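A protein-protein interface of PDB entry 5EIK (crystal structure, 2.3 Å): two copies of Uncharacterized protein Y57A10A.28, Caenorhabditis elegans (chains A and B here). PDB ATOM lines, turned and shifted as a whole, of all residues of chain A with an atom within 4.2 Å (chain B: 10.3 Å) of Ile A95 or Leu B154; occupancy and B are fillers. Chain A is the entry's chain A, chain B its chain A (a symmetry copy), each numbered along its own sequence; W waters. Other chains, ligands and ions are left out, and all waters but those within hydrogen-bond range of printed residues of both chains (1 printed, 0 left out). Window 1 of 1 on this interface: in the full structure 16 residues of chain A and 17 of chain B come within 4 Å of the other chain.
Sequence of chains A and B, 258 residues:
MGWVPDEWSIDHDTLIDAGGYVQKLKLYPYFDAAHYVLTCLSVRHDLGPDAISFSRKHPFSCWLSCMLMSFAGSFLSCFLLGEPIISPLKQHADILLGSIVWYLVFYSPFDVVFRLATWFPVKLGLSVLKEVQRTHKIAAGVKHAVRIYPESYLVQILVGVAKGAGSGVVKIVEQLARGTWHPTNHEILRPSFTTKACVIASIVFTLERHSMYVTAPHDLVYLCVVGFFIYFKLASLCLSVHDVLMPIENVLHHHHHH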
ATOM      1  N   TRP A  63      -3.706 -21.831 -22.962  1.00  0.00           N
ATOM      2  CA  TRP A  63      -2.541 -21.477 -22.168  1.00  0.00           C
ATOM      3  C   TRP A  63      -1.460 -20.863 -23.058  1.00  0.00           C
ATOM      4  O   TRP A  63      -0.864 -19.846 -22.707  1.00  0.00           O
ATOM      5  CB  TRP A  63      -1.968 -22.709 -21.471  1.00  0.00           C
ATOM      6  CG  TRP A  63      -0.638 -22.468 -20.835  1.00  0.00           C
ATOM      7  CD1 TRP A  63      -0.399 -21.862 -19.633  1.00  0.00           C
ATOM      8  CD2 TRP A  63       0.650 -22.769 -21.396  1.00  0.00           C
ATOM      9  NE1 TRP A  63       0.955 -21.765 -19.412  1.00  0.00           N
ATOM     10  CE2 TRP A  63       1.622 -22.313 -20.475  1.00  0.00           C
ATOM     11  CE3 TRP A  63       1.078 -23.377 -22.588  1.00  0.00           C
ATOM     12  CZ2 TRP A  63       3.000 -22.443 -20.706  1.00  0.00           C
ATOM     13  CZ3 TRP A  63       2.458 -23.510 -22.825  1.00  0.00           C
ATOM     14  CH2 TRP A  63       3.399 -23.041 -21.883  1.00  0.00           C
ATOM     15  N   PHE A  71       4.404 -12.610 -23.005  1.00  0.00           N
ATOM     16  CA  PHE A  71       5.833 -12.378 -23.186  1.00  0.00           C
ATOM     17  C   PHE A  71       6.180 -11.958 -24.611  1.00  0.00           C
ATOM     18  O   PHE A  71       7.316 -12.120 -25.065  1.00  0.00           O
ATOM     19  CB  PHE A  71       6.599 -13.646 -22.811  1.00  0.00           C
ATOM     20  CG  PHE A  71       6.449 -14.027 -21.372  1.00  0.00           C
ATOM     21  CD1 PHE A  71       7.126 -13.324 -20.378  1.00  0.00           C
ATOM     22  CD2 PHE A  71       5.581 -15.045 -21.000  1.00  0.00           C
ATOM     23  CE1 PHE A  71       6.932 -13.628 -19.023  1.00  0.00           C
ATOM     24  CE2 PHE A  71       5.378 -15.358 -19.653  1.00  0.00           C
ATOM     25  CZ  PHE A  71       6.056 -14.649 -18.662  1.00  0.00           C
ATOM     26  N   PRO A  88      12.838 -16.737 -23.562  1.00  0.00           N
ATOM     27  CA  PRO A  88      11.939 -16.271 -22.499  1.00  0.00           C
ATOM     28  C   PRO A  88      11.385 -17.348 -21.564  1.00  0.00           C
ATOM     29  O   PRO A  88      11.192 -17.096 -20.376  1.00  0.00           O
ATOM     30  CB  PRO A  88      10.837 -15.568 -23.278  1.00  0.00           C
ATOM     31  CG  PRO A  88      11.585 -14.994 -24.446  1.00  0.00           C
ATOM     32  CD  PRO A  88      12.458 -16.153 -24.863  1.00  0.00           C
ATOM     33  N   LEU A  89      11.132 -18.539 -22.103  1.00  0.00           N
ATOM     34  CA  LEU A  89      10.581 -19.650 -21.327  1.00  0.00           C
ATOM     35  C   LEU A  89      11.528 -20.214 -20.282  1.00  0.00           C
ATOM     36  O   LEU A  89      11.188 -21.160 -19.574  1.00  0.00           O
ATOM     37  CB  LEU A  89      10.150 -20.778 -22.259  1.00  0.00           C
ATOM     38  CG  LEU A  89       9.118 -20.398 -23.316  1.00  0.00           C
ATOM     39  CD1 LEU A  89       8.786 -21.623 -24.132  1.00  0.00           C
ATOM     40  CD2 LEU A  89       7.868 -19.841 -22.659  1.00  0.00           C
ATOM     41  N   GLN A  91      12.676 -18.340 -17.899  1.00  0.00           N
ATOM     42  CA  GLN A  91      12.462 -17.516 -16.720  1.00  0.00           C
ATOM     43  C   GLN A  91      11.346 -18.250 -15.994  1.00  0.00           C
ATOM     44  O   GLN A  91      10.194 -17.824 -16.006  1.00  0.00           O
ATOM     45  CB  GLN A  91      11.994 -16.115 -17.120  1.00  0.00           C
ATOM     46  CG  GLN A  91      12.873 -15.433 -18.158  1.00  0.00           C
ATOM     47  CD  GLN A  91      14.274 -15.146 -17.651  1.00  0.00           C
ATOM     48  OE1 GLN A  91      14.457 -14.427 -16.666  1.00  0.00           O
ATOM     49  NE2 GLN A  91      15.274 -15.706 -18.324  1.00  0.00           N
ATOM     50  N   HIS A  92      11.708 -19.372 -15.382  1.00  0.00           N
ATOM     51  CA  HIS A  92      10.776 -20.230 -14.668  1.00  0.00           C
ATOM     52  C   HIS A  92       9.795 -19.504 -13.766  1.00  0.00           C
ATOM     53  O   HIS A  92       8.588 -19.711 -13.868  1.00  0.00           O
ATOM     54  CB  HIS A  92      11.558 -21.283 -13.885  1.00  0.00           C
ATOM     55  CG  HIS A  92      12.453 -22.118 -14.748  1.00  0.00           C
ATOM     56  ND1 HIS A  92      13.576 -21.609 -15.368  1.00  0.00           N
ATOM     57  CD2 HIS A  92      12.369 -23.414 -15.137  1.00  0.00           C
ATOM     58  CE1 HIS A  92      14.140 -22.552 -16.101  1.00  0.00           C
ATOM     59  NE2 HIS A  92      13.427 -23.657 -15.978  1.00  0.00           N
ATOM     60  N   ALA A  93      10.303 -18.648 -12.891  1.00  0.00           N
ATOM     61  CA  ALA A  93       9.430 -17.896 -11.999  1.00  0.00           C
ATOM     62  C   ALA A  93       8.377 -17.123 -12.803  1.00  0.00           C
ATOM     63  O   ALA A  93       7.188 -17.151 -12.463  1.00  0.00           O
ATOM     64  CB  ALA A  93      10.254 -16.929 -11.135  1.00  0.00           C
ATOM     65  N   ASP A  94       8.813 -16.443 -13.862  1.00  0.00           N
ATOM     66  CA  ASP A  94       7.896 -15.669 -14.703  1.00  0.00           C
ATOM     67  C   ASP A  94       6.832 -16.536 -15.353  1.00  0.00           C
ATOM     68  O   ASP A  94       5.643 -16.215 -15.300  1.00  0.00           O
ATOM     69  CB  ASP A  94       8.650 -14.927 -15.811  1.00  0.00           C
ATOM     70  CG  ASP A  94       9.510 -13.809 -15.286  1.00  0.00           C
ATOM     71  OD1 ASP A  94       9.195 -13.267 -14.203  1.00  0.00           O
ATOM     72  OD2 ASP A  94      10.496 -13.464 -15.968  1.00  0.00           O
ATOM     73  N   ILE A  95       7.263 -17.632 -15.970  1.00  0.00           N
ATOM     74  CA  ILE A  95       6.334 -18.533 -16.638  1.00  0.00           C
ATOM     75  C   ILE A  95       5.353 -19.138 -15.651  1.00  0.00           C
ATOM     76  O   ILE A  95       4.172 -19.313 -15.967  1.00  0.00           O
ATOM     77  CB  ILE A  95       7.081 -19.661 -17.369  1.00  0.00           C
ATOM     78  CG1 ILE A  95       8.052 -19.056 -18.376  1.00  0.00           C
ATOM     79  CG2 ILE A  95       6.101 -20.570 -18.082  1.00  0.00           C
ATOM     80  CD1 ILE A  95       7.399 -18.093 -19.343  1.00  0.00           C
ATOM     81  N   LEU A  96       5.830 -19.453 -14.452  1.00  0.00           N
ATOM     82  CA  LEU A  96       4.939 -20.024 -13.451  1.00  0.00           C
ATOM     83  C   LEU A  96       3.888 -18.999 -13.045  1.00  0.00           C
ATOM     84  O   LEU A  96       2.694 -19.298 -13.054  1.00  0.00           O
ATOM     85  CB  LEU A  96       5.704 -20.474 -12.212  1.00  0.00           C
ATOM     86  CG  LEU A  96       4.766 -21.068 -11.157  1.00  0.00           C
ATOM     87  CD1 LEU A  96       4.030 -22.280 -11.713  1.00  0.00           C
ATOM     88  CD2 LEU A  96       5.557 -21.469  -9.962  1.00  0.00           C
ATOM     89  N   LEU A  97       4.329 -17.787 -12.708  1.00  0.00           N
ATOM     90  CA  LEU A  97       3.403 -16.733 -12.307  1.00  0.00           C
ATOM     91  C   LEU A  97       2.402 -16.462 -13.434  1.00  0.00           C
ATOM     92  O   LEU A  97       1.210 -16.272 -13.188  1.00  0.00           O
ATOM     93  CB  LEU A  97       4.162 -15.443 -11.950  1.00  0.00           C
ATOM     94  CG  LEU A  97       3.321 -14.219 -11.538  1.00  0.00           C
ATOM     95  CD1 LEU A  97       2.461 -14.533 -10.329  1.00  0.00           C
ATOM     96  CD2 LEU A  97       4.224 -13.042 -11.228  1.00  0.00           C
ATOM     97  N   GLY A  98       2.895 -16.459 -14.671  1.00  0.00           N
ATOM     98  CA  GLY A  98       2.034 -16.223 -15.812  1.00  0.00           C
ATOM     99  C   GLY A  98       1.000 -17.319 -15.999  1.00  0.00           C
ATOM    100  O   GLY A  98      -0.163 -17.052 -16.310  1.00  0.00           O
ATOM    101  N   SER A  99       1.419 -18.561 -15.816  1.00  0.00           N
ATOM    102  CA  SER A  99       0.496 -19.682 -15.957  1.00  0.00           C
ATOM    103  C   SER A  99      -0.557 -19.672 -14.840  1.00  0.00           C
ATOM    104  O   SER A  99      -1.727 -20.011 -15.066  1.00  0.00           O
ATOM    105  CB  SER A  99       1.269 -20.995 -15.924  1.00  0.00           C
ATOM    106  OG  SER A  99       2.316 -20.962 -16.870  1.00  0.00           O
ATOM    107  N   LEU B  80      12.409 -22.272 -33.263  1.00  0.00           N
ATOM    108  CA  LEU B  80      12.303 -22.124 -31.816  1.00  0.00           C
ATOM    109  C   LEU B  80      13.645 -22.109 -31.094  1.00  0.00           C
ATOM    110  O   LEU B  80      13.829 -21.369 -30.127  1.00  0.00           O
ATOM    111  CB  LEU B  80      11.441 -23.244 -31.229  1.00  0.00           C
ATOM    112  CG  LEU B  80      10.008 -23.351 -31.754  1.00  0.00           C
ATOM    113  CD1 LEU B  80       9.335 -24.517 -31.064  1.00  0.00           C
ATOM    114  CD2 LEU B  80       9.245 -22.050 -31.501  1.00  0.00           C
ATOM    115  N   LEU B  81      14.584 -22.920 -31.565  1.00  0.00           N
ATOM    116  CA  LEU B  81      15.895 -23.010 -30.934  1.00  0.00           C
ATOM    117  C   LEU B  81      16.920 -22.000 -31.430  1.00  0.00           C
ATOM    118  O   LEU B  81      18.035 -21.946 -30.922  1.00  0.00           O
ATOM    119  CB  LEU B  81      16.441 -24.428 -31.100  1.00  0.00           C
ATOM    120  CG  LEU B  81      15.551 -25.480 -30.430  1.00  0.00           C
ATOM    121  CD1 LEU B  81      16.029 -26.877 -30.796  1.00  0.00           C
ATOM    122  CD2 LEU B  81      15.559 -25.269 -28.917  1.00  0.00           C
ATOM    123  N   GLY B 141      12.861 -34.887 -30.992  1.00  0.00           N
ATOM    124  CA  GLY B 141      12.786 -33.480 -30.655  1.00  0.00           C
ATOM    125  C   GLY B 141      13.038 -33.255 -29.176  1.00  0.00           C
ATOM    126  O   GLY B 141      13.768 -32.337 -28.791  1.00  0.00           O
ATOM    127  N   VAL B 142      12.434 -34.105 -28.348  1.00  0.00           N
ATOM    128  CA  VAL B 142      12.592 -34.010 -26.906  1.00  0.00           C
ATOM    129  C   VAL B 142      14.043 -34.268 -26.508  1.00  0.00           C
ATOM    130  O   VAL B 142      14.620 -33.531 -25.703  1.00  0.00           O
ATOM    131  CB  VAL B 142      11.662 -35.015 -26.190  1.00  0.00           C
ATOM    132  CG1 VAL B 142      12.015 -35.107 -24.722  1.00  0.00           C
ATOM    133  CG2 VAL B 142      10.214 -34.569 -26.347  1.00  0.00           C
ATOM    134  N   ALA B 145      16.232 -31.303 -27.436  1.00  0.00           N
ATOM    135  CA  ALA B 145      16.021 -30.202 -26.504  1.00  0.00           C
ATOM    136  C   ALA B 145      16.664 -30.466 -25.149  1.00  0.00           C
ATOM    137  O   ALA B 145      17.208 -29.553 -24.527  1.00  0.00           O
ATOM    138  CB  ALA B 145      14.533 -29.937 -26.324  1.00  0.00           C
ATOM    139  N   VAL B 146      16.592 -31.711 -24.690  1.00  0.00           N
ATOM    140  CA  VAL B 146      17.170 -32.087 -23.405  1.00  0.00           C
ATOM    141  C   VAL B 146      18.683 -31.900 -23.396  1.00  0.00           C
ATOM    142  O   VAL B 146      19.264 -31.487 -22.393  1.00  0.00           O
ATOM    143  CB  VAL B 146      16.834 -33.557 -23.069  1.00  0.00           C
ATOM    144  CG1 VAL B 146      17.648 -34.030 -21.871  1.00  0.00           C
ATOM    145  CG2 VAL B 146      15.356 -33.672 -22.769  1.00  0.00           C
ATOM    146  N   TYR B 149      19.046 -27.778 -23.426  1.00  0.00           N
ATOM    147  CA  TYR B 149      18.525 -27.129 -22.222  1.00  0.00           C
ATOM    148  C   TYR B 149      18.066 -28.181 -21.217  1.00  0.00           C
ATOM    149  O   TYR B 149      16.867 -28.391 -21.013  1.00  0.00           O
ATOM    150  CB  TYR B 149      17.359 -26.214 -22.598  1.00  0.00           C
ATOM    151  CG  TYR B 149      17.758 -25.140 -23.572  1.00  0.00           C
ATOM    152  CD1 TYR B 149      18.527 -24.054 -23.160  1.00  0.00           C
ATOM    153  CD2 TYR B 149      17.415 -25.234 -24.919  1.00  0.00           C
ATOM    154  CE1 TYR B 149      18.952 -23.088 -24.066  1.00  0.00           C
ATOM    155  CE2 TYR B 149      17.833 -24.273 -25.834  1.00  0.00           C
ATOM    156  CZ  TYR B 149      18.605 -23.204 -25.402  1.00  0.00           C
ATOM    157  OH  TYR B 149      19.045 -22.264 -26.304  1.00  0.00           O
ATOM    158  N   PRO B 150      19.025 -28.838 -20.556  1.00  0.00           N
ATOM    159  CA  PRO B 150      18.782 -29.887 -19.564  1.00  0.00           C
ATOM    160  C   PRO B 150      17.699 -29.644 -18.510  1.00  0.00           C
ATOM    161  O   PRO B 150      17.008 -30.579 -18.123  1.00  0.00           O
ATOM    162  CB  PRO B 150      20.160 -30.087 -18.937  1.00  0.00           C
ATOM    163  CG  PRO B 150      21.094 -29.752 -20.059  1.00  0.00           C
ATOM    164  CD  PRO B 150      20.460 -28.502 -20.607  1.00  0.00           C
ATOM    165  N   GLU B 151      17.530 -28.408 -18.052  1.00  0.00           N
ATOM    166  CA  GLU B 151      16.537 -28.151 -17.008  1.00  0.00           C
ATOM    167  C   GLU B 151      15.249 -27.454 -17.443  1.00  0.00           C
ATOM    168  O   GLU B 151      14.381 -27.171 -16.617  1.00  0.00           O
ATOM    169  CB  GLU B 151      17.187 -27.350 -15.878  1.00  0.00           C
ATOM    170  CG  GLU B 151      18.594 -27.814 -15.532  1.00  0.00           C
ATOM    171  CD  GLU B 151      18.662 -29.292 -15.186  1.00  0.00           C
ATOM    172  OE1 GLU B 151      19.785 -29.842 -15.151  1.00  0.00           O
ATOM    173  OE2 GLU B 151      17.597 -29.903 -14.943  1.00  0.00           O
ATOM    174  N   SER B 152      15.115 -27.181 -18.735  1.00  0.00           N
ATOM    175  CA  SER B 152      13.928 -26.499 -19.226  1.00  0.00           C
ATOM    176  C   SER B 152      12.880 -27.486 -19.716  1.00  0.00           C
ATOM    177  O   SER B 152      12.810 -27.779 -20.908  1.00  0.00           O
ATOM    178  CB  SER B 152      14.313 -25.541 -20.350  1.00  0.00           C
ATOM    179  OG  SER B 152      15.375 -24.694 -19.944  1.00  0.00           O
ATOM    180  N   TYR B 153      12.074 -27.991 -18.790  1.00  0.00           N
ATOM    181  CA  TYR B 153      11.025 -28.950 -19.110  1.00  0.00           C
ATOM    182  C   TYR B 153      10.042 -28.429 -20.154  1.00  0.00           C
ATOM    183  O   TYR B 153       9.613 -29.164 -21.045  1.00  0.00           O
ATOM    184  CB  TYR B 153      10.239 -29.319 -17.848  1.00  0.00           C
ATOM    185  CG  TYR B 153      10.898 -30.342 -16.950  1.00  0.00           C
ATOM    186  CD1 TYR B 153      12.220 -30.191 -16.528  1.00  0.00           C
ATOM    187  CD2 TYR B 153      10.173 -31.437 -16.467  1.00  0.00           C
ATOM    188  CE1 TYR B 153      12.801 -31.098 -15.643  1.00  0.00           C
ATOM    189  CE2 TYR B 153      10.742 -32.349 -15.584  1.00  0.00           C
ATOM    190  CZ  TYR B 153      12.055 -32.174 -15.174  1.00  0.00           C
ATOM    191  OH  TYR B 153      12.612 -33.064 -14.285  1.00  0.00           O
ATOM    192  N   LEU B 154       9.679 -27.158 -20.028  1.00  0.00           N
ATOM    193  CA  LEU B 154       8.734 -26.543 -20.940  1.00  0.00           C
ATOM    194  C   LEU B 154       9.279 -26.498 -22.362  1.00  0.00           C
ATOM    195  O   LEU B 154       8.595 -26.891 -23.299  1.00  0.00           O
ATOM    196  CB  LEU B 154       8.400 -25.139 -20.458  1.00  0.00           C
ATOM    197  CG  LEU B 154       7.133 -24.525 -21.047  1.00  0.00           C
ATOM    198  CD1 LEU B 154       6.001 -25.541 -20.999  1.00  0.00           C
ATOM    199  CD2 LEU B 154       6.776 -23.275 -20.255  1.00  0.00           C
ATOM    200  N   VAL B 155      10.508 -26.015 -22.517  1.00  0.00           N
ATOM    201  CA  VAL B 155      11.126 -25.949 -23.831  1.00  0.00           C
ATOM    202  C   VAL B 155      11.172 -27.349 -24.458  1.00  0.00           C
ATOM    203  O   VAL B 155      10.858 -27.526 -25.639  1.00  0.00           O
ATOM    204  CB  VAL B 155      12.558 -25.392 -23.746  1.00  0.00           C
ATOM    205  CG1 VAL B 155      13.221 -25.446 -25.107  1.00  0.00           C
ATOM    206  CG2 VAL B 155      12.525 -23.961 -23.252  1.00  0.00           C
ATOM    207  N   GLN B 156      11.556 -28.337 -23.655  1.00  0.00           N
ATOM    208  CA  GLN B 156      11.637 -29.711 -24.112  1.00  0.00           C
ATOM    209  C   GLN B 156      10.287 -30.187 -24.655  1.00  0.00           C
ATOM    210  O   GLN B 156      10.214 -30.823 -25.704  1.00  0.00           O
ATOM    211  CB  GLN B 156      12.090 -30.601 -22.962  1.00  0.00           C
ATOM    212  CG  GLN B 156      13.528 -30.345 -22.523  1.00  0.00           C
ATOM    213  CD  GLN B 156      13.828 -30.920 -21.151  1.00  0.00           C
ATOM    214  OE1 GLN B 156      13.082 -31.760 -20.648  1.00  0.00           O
ATOM    215  NE2 GLN B 156      14.919 -30.477 -20.544  1.00  0.00           N
ATOM    216  N   ILE B 157       9.215 -29.866 -23.945  1.00  0.00           N
ATOM    217  CA  ILE B 157       7.900 -30.280 -24.384  1.00  0.00           C
ATOM    218  C   ILE B 157       7.499 -29.566 -25.675  1.00  0.00           C
ATOM    219  O   ILE B 157       7.095 -30.208 -26.645  1.00  0.00           O
ATOM    220  CB  ILE B 157       6.856 -30.026 -23.278  1.00  0.00           C
ATOM    221  CG1 ILE B 157       7.166 -30.915 -22.074  1.00  0.00           C
ATOM    222  CG2 ILE B 157       5.464 -30.357 -23.769  1.00  0.00           C
ATOM    223  CD1 ILE B 157       6.333 -30.583 -20.838  1.00  0.00           C
ATOM    224  N   LEU B 158       7.631 -28.245 -25.696  1.00  0.00           N
ATOM    225  CA  LEU B 158       7.265 -27.475 -26.877  1.00  0.00           C
ATOM    226  C   LEU B 158       8.034 -27.914 -28.121  1.00  0.00           C
ATOM    227  O   LEU B 158       7.468 -28.004 -29.211  1.00  0.00           O
ATOM    228  CB  LEU B 158       7.470 -25.983 -26.607  1.00  0.00           C
ATOM    229  CG  LEU B 158       6.597 -25.483 -25.455  1.00  0.00           C
ATOM    230  CD1 LEU B 158       6.927 -24.034 -25.140  1.00  0.00           C
ATOM    231  CD2 LEU B 158       5.123 -25.649 -25.827  1.00  0.00           C
ATOM    232  N   VAL B 159       9.322 -28.191 -27.962  1.00  0.00           N
ATOM    233  CA  VAL B 159      10.115 -28.637 -29.095  1.00  0.00           C
ATOM    234  C   VAL B 159       9.565 -29.978 -29.605  1.00  0.00           C
ATOM    235  O   VAL B 159       9.444 -30.193 -30.813  1.00  0.00           O
ATOM    236  CB  VAL B 159      11.608 -28.775 -28.709  1.00  0.00           C
ATOM    237  CG1 VAL B 159      12.370 -29.536 -29.793  1.00  0.00           C
ATOM    238  CG2 VAL B 159      12.217 -27.387 -28.531  1.00  0.00           C
ATOM    239  N   GLY B 160       9.216 -30.866 -28.676  1.00  0.00           N
ATOM    240  CA  GLY B 160       8.677 -32.152 -29.052  1.00  0.00           C
ATOM    241  C   GLY B 160       7.392 -31.982 -29.839  1.00  0.00           C
ATOM    242  O   GLY B 160       7.159 -32.672 -30.838  1.00  0.00           O
ATOM    243  N   VAL B 161       6.551 -31.057 -29.388  1.00  0.00           N
ATOM    244  CA  VAL B 161       5.286 -30.791 -30.058  1.00  0.00           C
ATOM    245  C   VAL B 161       5.527 -30.159 -31.431  1.00  0.00           C
ATOM    246  O   VAL B 161       4.829 -30.472 -32.399  1.00  0.00           O
ATOM    247  CB  VAL B 161       4.407 -29.856 -29.201  1.00  0.00           C
ATOM    248  CG1 VAL B 161       3.106 -29.548 -29.913  1.00  0.00           C
ATOM    249  CG2 VAL B 161       4.118 -30.510 -27.861  1.00  0.00           C
ATOM    250  N   ALA B 162       6.521 -29.280 -31.513  1.00  0.00           N
ATOM    251  CA  ALA B 162       6.841 -28.608 -32.771  1.00  0.00           C
ATOM    252  C   ALA B 162       7.262 -29.628 -33.818  1.00  0.00           C
ATOM    253  O   ALA B 162       6.878 -29.525 -34.980  1.00  0.00           O
ATOM    254  CB  ALA B 162       7.952 -27.573 -32.560  1.00  0.00           C
ATOM    255  N   VAL B 199       1.016 -33.259 -27.872  1.00  0.00           N
ATOM    256  CA  VAL B 199       1.304 -32.582 -26.610  1.00  0.00           C
ATOM    257  C   VAL B 199       1.480 -33.640 -25.536  1.00  0.00           C
ATOM    258  O   VAL B 199       2.488 -33.650 -24.820  1.00  0.00           O
ATOM    259  CB  VAL B 199       0.164 -31.607 -26.208  1.00  0.00           C
ATOM    260  CG1 VAL B 199       0.417 -31.027 -24.811  1.00  0.00           C
ATOM    261  CG2 VAL B 199       0.083 -30.467 -27.223  1.00  0.00           C
ATOM    262  N   SER B 202       4.535 -35.702 -26.072  1.00  0.00           N
ATOM    263  CA  SER B 202       5.715 -34.909 -25.749  1.00  0.00           C
ATOM    264  C   SER B 202       5.954 -34.822 -24.246  1.00  0.00           C
ATOM    265  O   SER B 202       7.086 -34.974 -23.774  1.00  0.00           O
ATOM    266  CB  SER B 202       5.583 -33.504 -26.338  1.00  0.00           C
ATOM    267  OG  SER B 202       6.806 -32.810 -26.233  1.00  0.00           O
ATOM    268  N   ILE B 203       4.888 -34.565 -23.496  1.00  0.00           N
ATOM    269  CA  ILE B 203       4.984 -34.487 -22.044  1.00  0.00           C
ATOM    270  C   ILE B 203       5.505 -35.829 -21.521  1.00  0.00           C
ATOM    271  O   ILE B 203       6.457 -35.886 -20.737  1.00  0.00           O
ATOM    272  CB  ILE B 203       3.604 -34.198 -21.417  1.00  0.00           C
ATOM    273  CG1 ILE B 203       3.233 -32.734 -21.637  1.00  0.00           C
ATOM    274  CG2 ILE B 203       3.606 -34.566 -19.937  1.00  0.00           C
ATOM    275  CD1 ILE B 203       1.815 -32.404 -21.231  1.00  0.00           C
ATOM    276  N   THR B 206       9.076 -36.397 -22.176  1.00  0.00           N
ATOM    277  CA  THR B 206       9.882 -35.487 -21.386  1.00  0.00           C
ATOM    278  C   THR B 206      10.003 -36.069 -19.990  1.00  0.00           C
ATOM    279  O   THR B 206      11.110 -36.204 -19.458  1.00  0.00           O
ATOM    280  CB  THR B 206       9.247 -34.087 -21.321  1.00  0.00           C
ATOM    281  OG1 THR B 206       9.255 -33.508 -22.632  1.00  0.00           O
ATOM    282  CG2 THR B 206      10.028 -33.183 -20.377  1.00  0.00           C
ATOM    283  N   LEU B 207       8.862 -36.422 -19.406  1.00  0.00           N
ATOM    284  CA  LEU B 207       8.841 -37.013 -18.068  1.00  0.00           C
ATOM    285  C   LEU B 207       9.721 -38.253 -18.048  1.00  0.00           C
ATOM    286  O   LEU B 207      10.535 -38.455 -17.141  1.00  0.00           O
ATOM    287  CB  LEU B 207       7.418 -37.411 -17.681  1.00  0.00           C
ATOM    288  CG  LEU B 207       6.440 -36.278 -17.386  1.00  0.00           C
ATOM    289  CD1 LEU B 207       5.087 -36.867 -17.046  1.00  0.00           C
ATOM    290  CD2 LEU B 207       6.963 -35.434 -16.234  1.00  0.00           C
ATOM    291  N   HIS B 210      13.247 -37.667 -17.691  1.00  0.00           N
ATOM    292  CA  HIS B 210      13.670 -37.216 -16.376  1.00  0.00           C
ATOM    293  C   HIS B 210      13.299 -38.249 -15.326  1.00  0.00           C
ATOM    294  O   HIS B 210      13.354 -37.980 -14.126  1.00  0.00           O
ATOM    295  CB  HIS B 210      13.030 -35.864 -16.060  1.00  0.00           C
ATOM    296  CG  HIS B 210      13.560 -34.742 -16.894  1.00  0.00           C
ATOM    297  ND1 HIS B 210      14.838 -34.246 -16.746  1.00  0.00           N
ATOM    298  CD2 HIS B 210      13.003 -34.045 -17.913  1.00  0.00           C
ATOM    299  CE1 HIS B 210      15.044 -33.294 -17.637  1.00  0.00           C
ATOM    300  NE2 HIS B 210      13.946 -33.152 -18.359  1.00  0.00           N
HETATM  301  O   HOH W   1      11.517 -24.481 -19.433  1.00  0.00           O
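Of chain B, only Leu B154 (3.5 Å) comes within 4 Å of Ile A95. Of chain A, only Trp A63 (3.7 Å) and Ile A95 (3.5 Å) come within 4 Å of Leu B154. No residue of chain B comes within 4 Å of Ala A93. No residue of chain B comes within 4 Å of Gly A98. Printed residues of chain A within 4 Å of Glu B151: His A92. Printed residues of chain A within 4 Å of Leu B158: Leu A89 (3.2 Å). Of the printed residues of chain B, His A92 touches Glu B151. Of the printed residues of chain B, Trp A63 touches Leu B154 (3.7 Å). Gly B141 touches none of the printed residues of chain A. Leu B80 touches none of the printed residues of chain A. The nearest residue of chain B that does not touch Ile A95 is Leu B158 (7.9 Å). The nearest printed residue of chain A that does not touch Leu B154 is Leu A89 (4.3 Å).
No position is printed for both chains.
The indole nitrogen (NE1) of Trp A63 is in hydrogen-bond range of the side-chain hydroxyl (OG) of Ser A99 (3.0 Å). The backbone carbonyl oxygen (O) of Ile A95 sits at hydrogen-bond distance from the side-chain hydroxyl (OG) of Ser A99 (2.6 Å).
Of the 13 printed residues of chain A, 4 touch a printed residue of chain B. Hydrophobic or aromatic side chains of chain A that line the printed part of chain B: Trp A63, Leu A89, His A92 and Ile A95. Along chain A the printed residues that touch a printed residue of chain B span positions 63 to 95. Of the 26 printed residues of chain B, 3 touch a printed residue of chain A. Hydrophobic or aromatic side chains of chain B that line the printed part of chain A: Leu B154 and Leu B158.
Water W1 lies within hydrogen-bond range of the backbone NH of Leu B154 (3.3 Å) and the backbone carbonyl oxygen of Leu A89 (3.3 Å).
Among the printed residues, pairs that only touch across the chains: Trp A63 with Leu B154, Leu A89 with Leu B158, His A92 with Glu B151 and Ile A95 with Leu B154.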
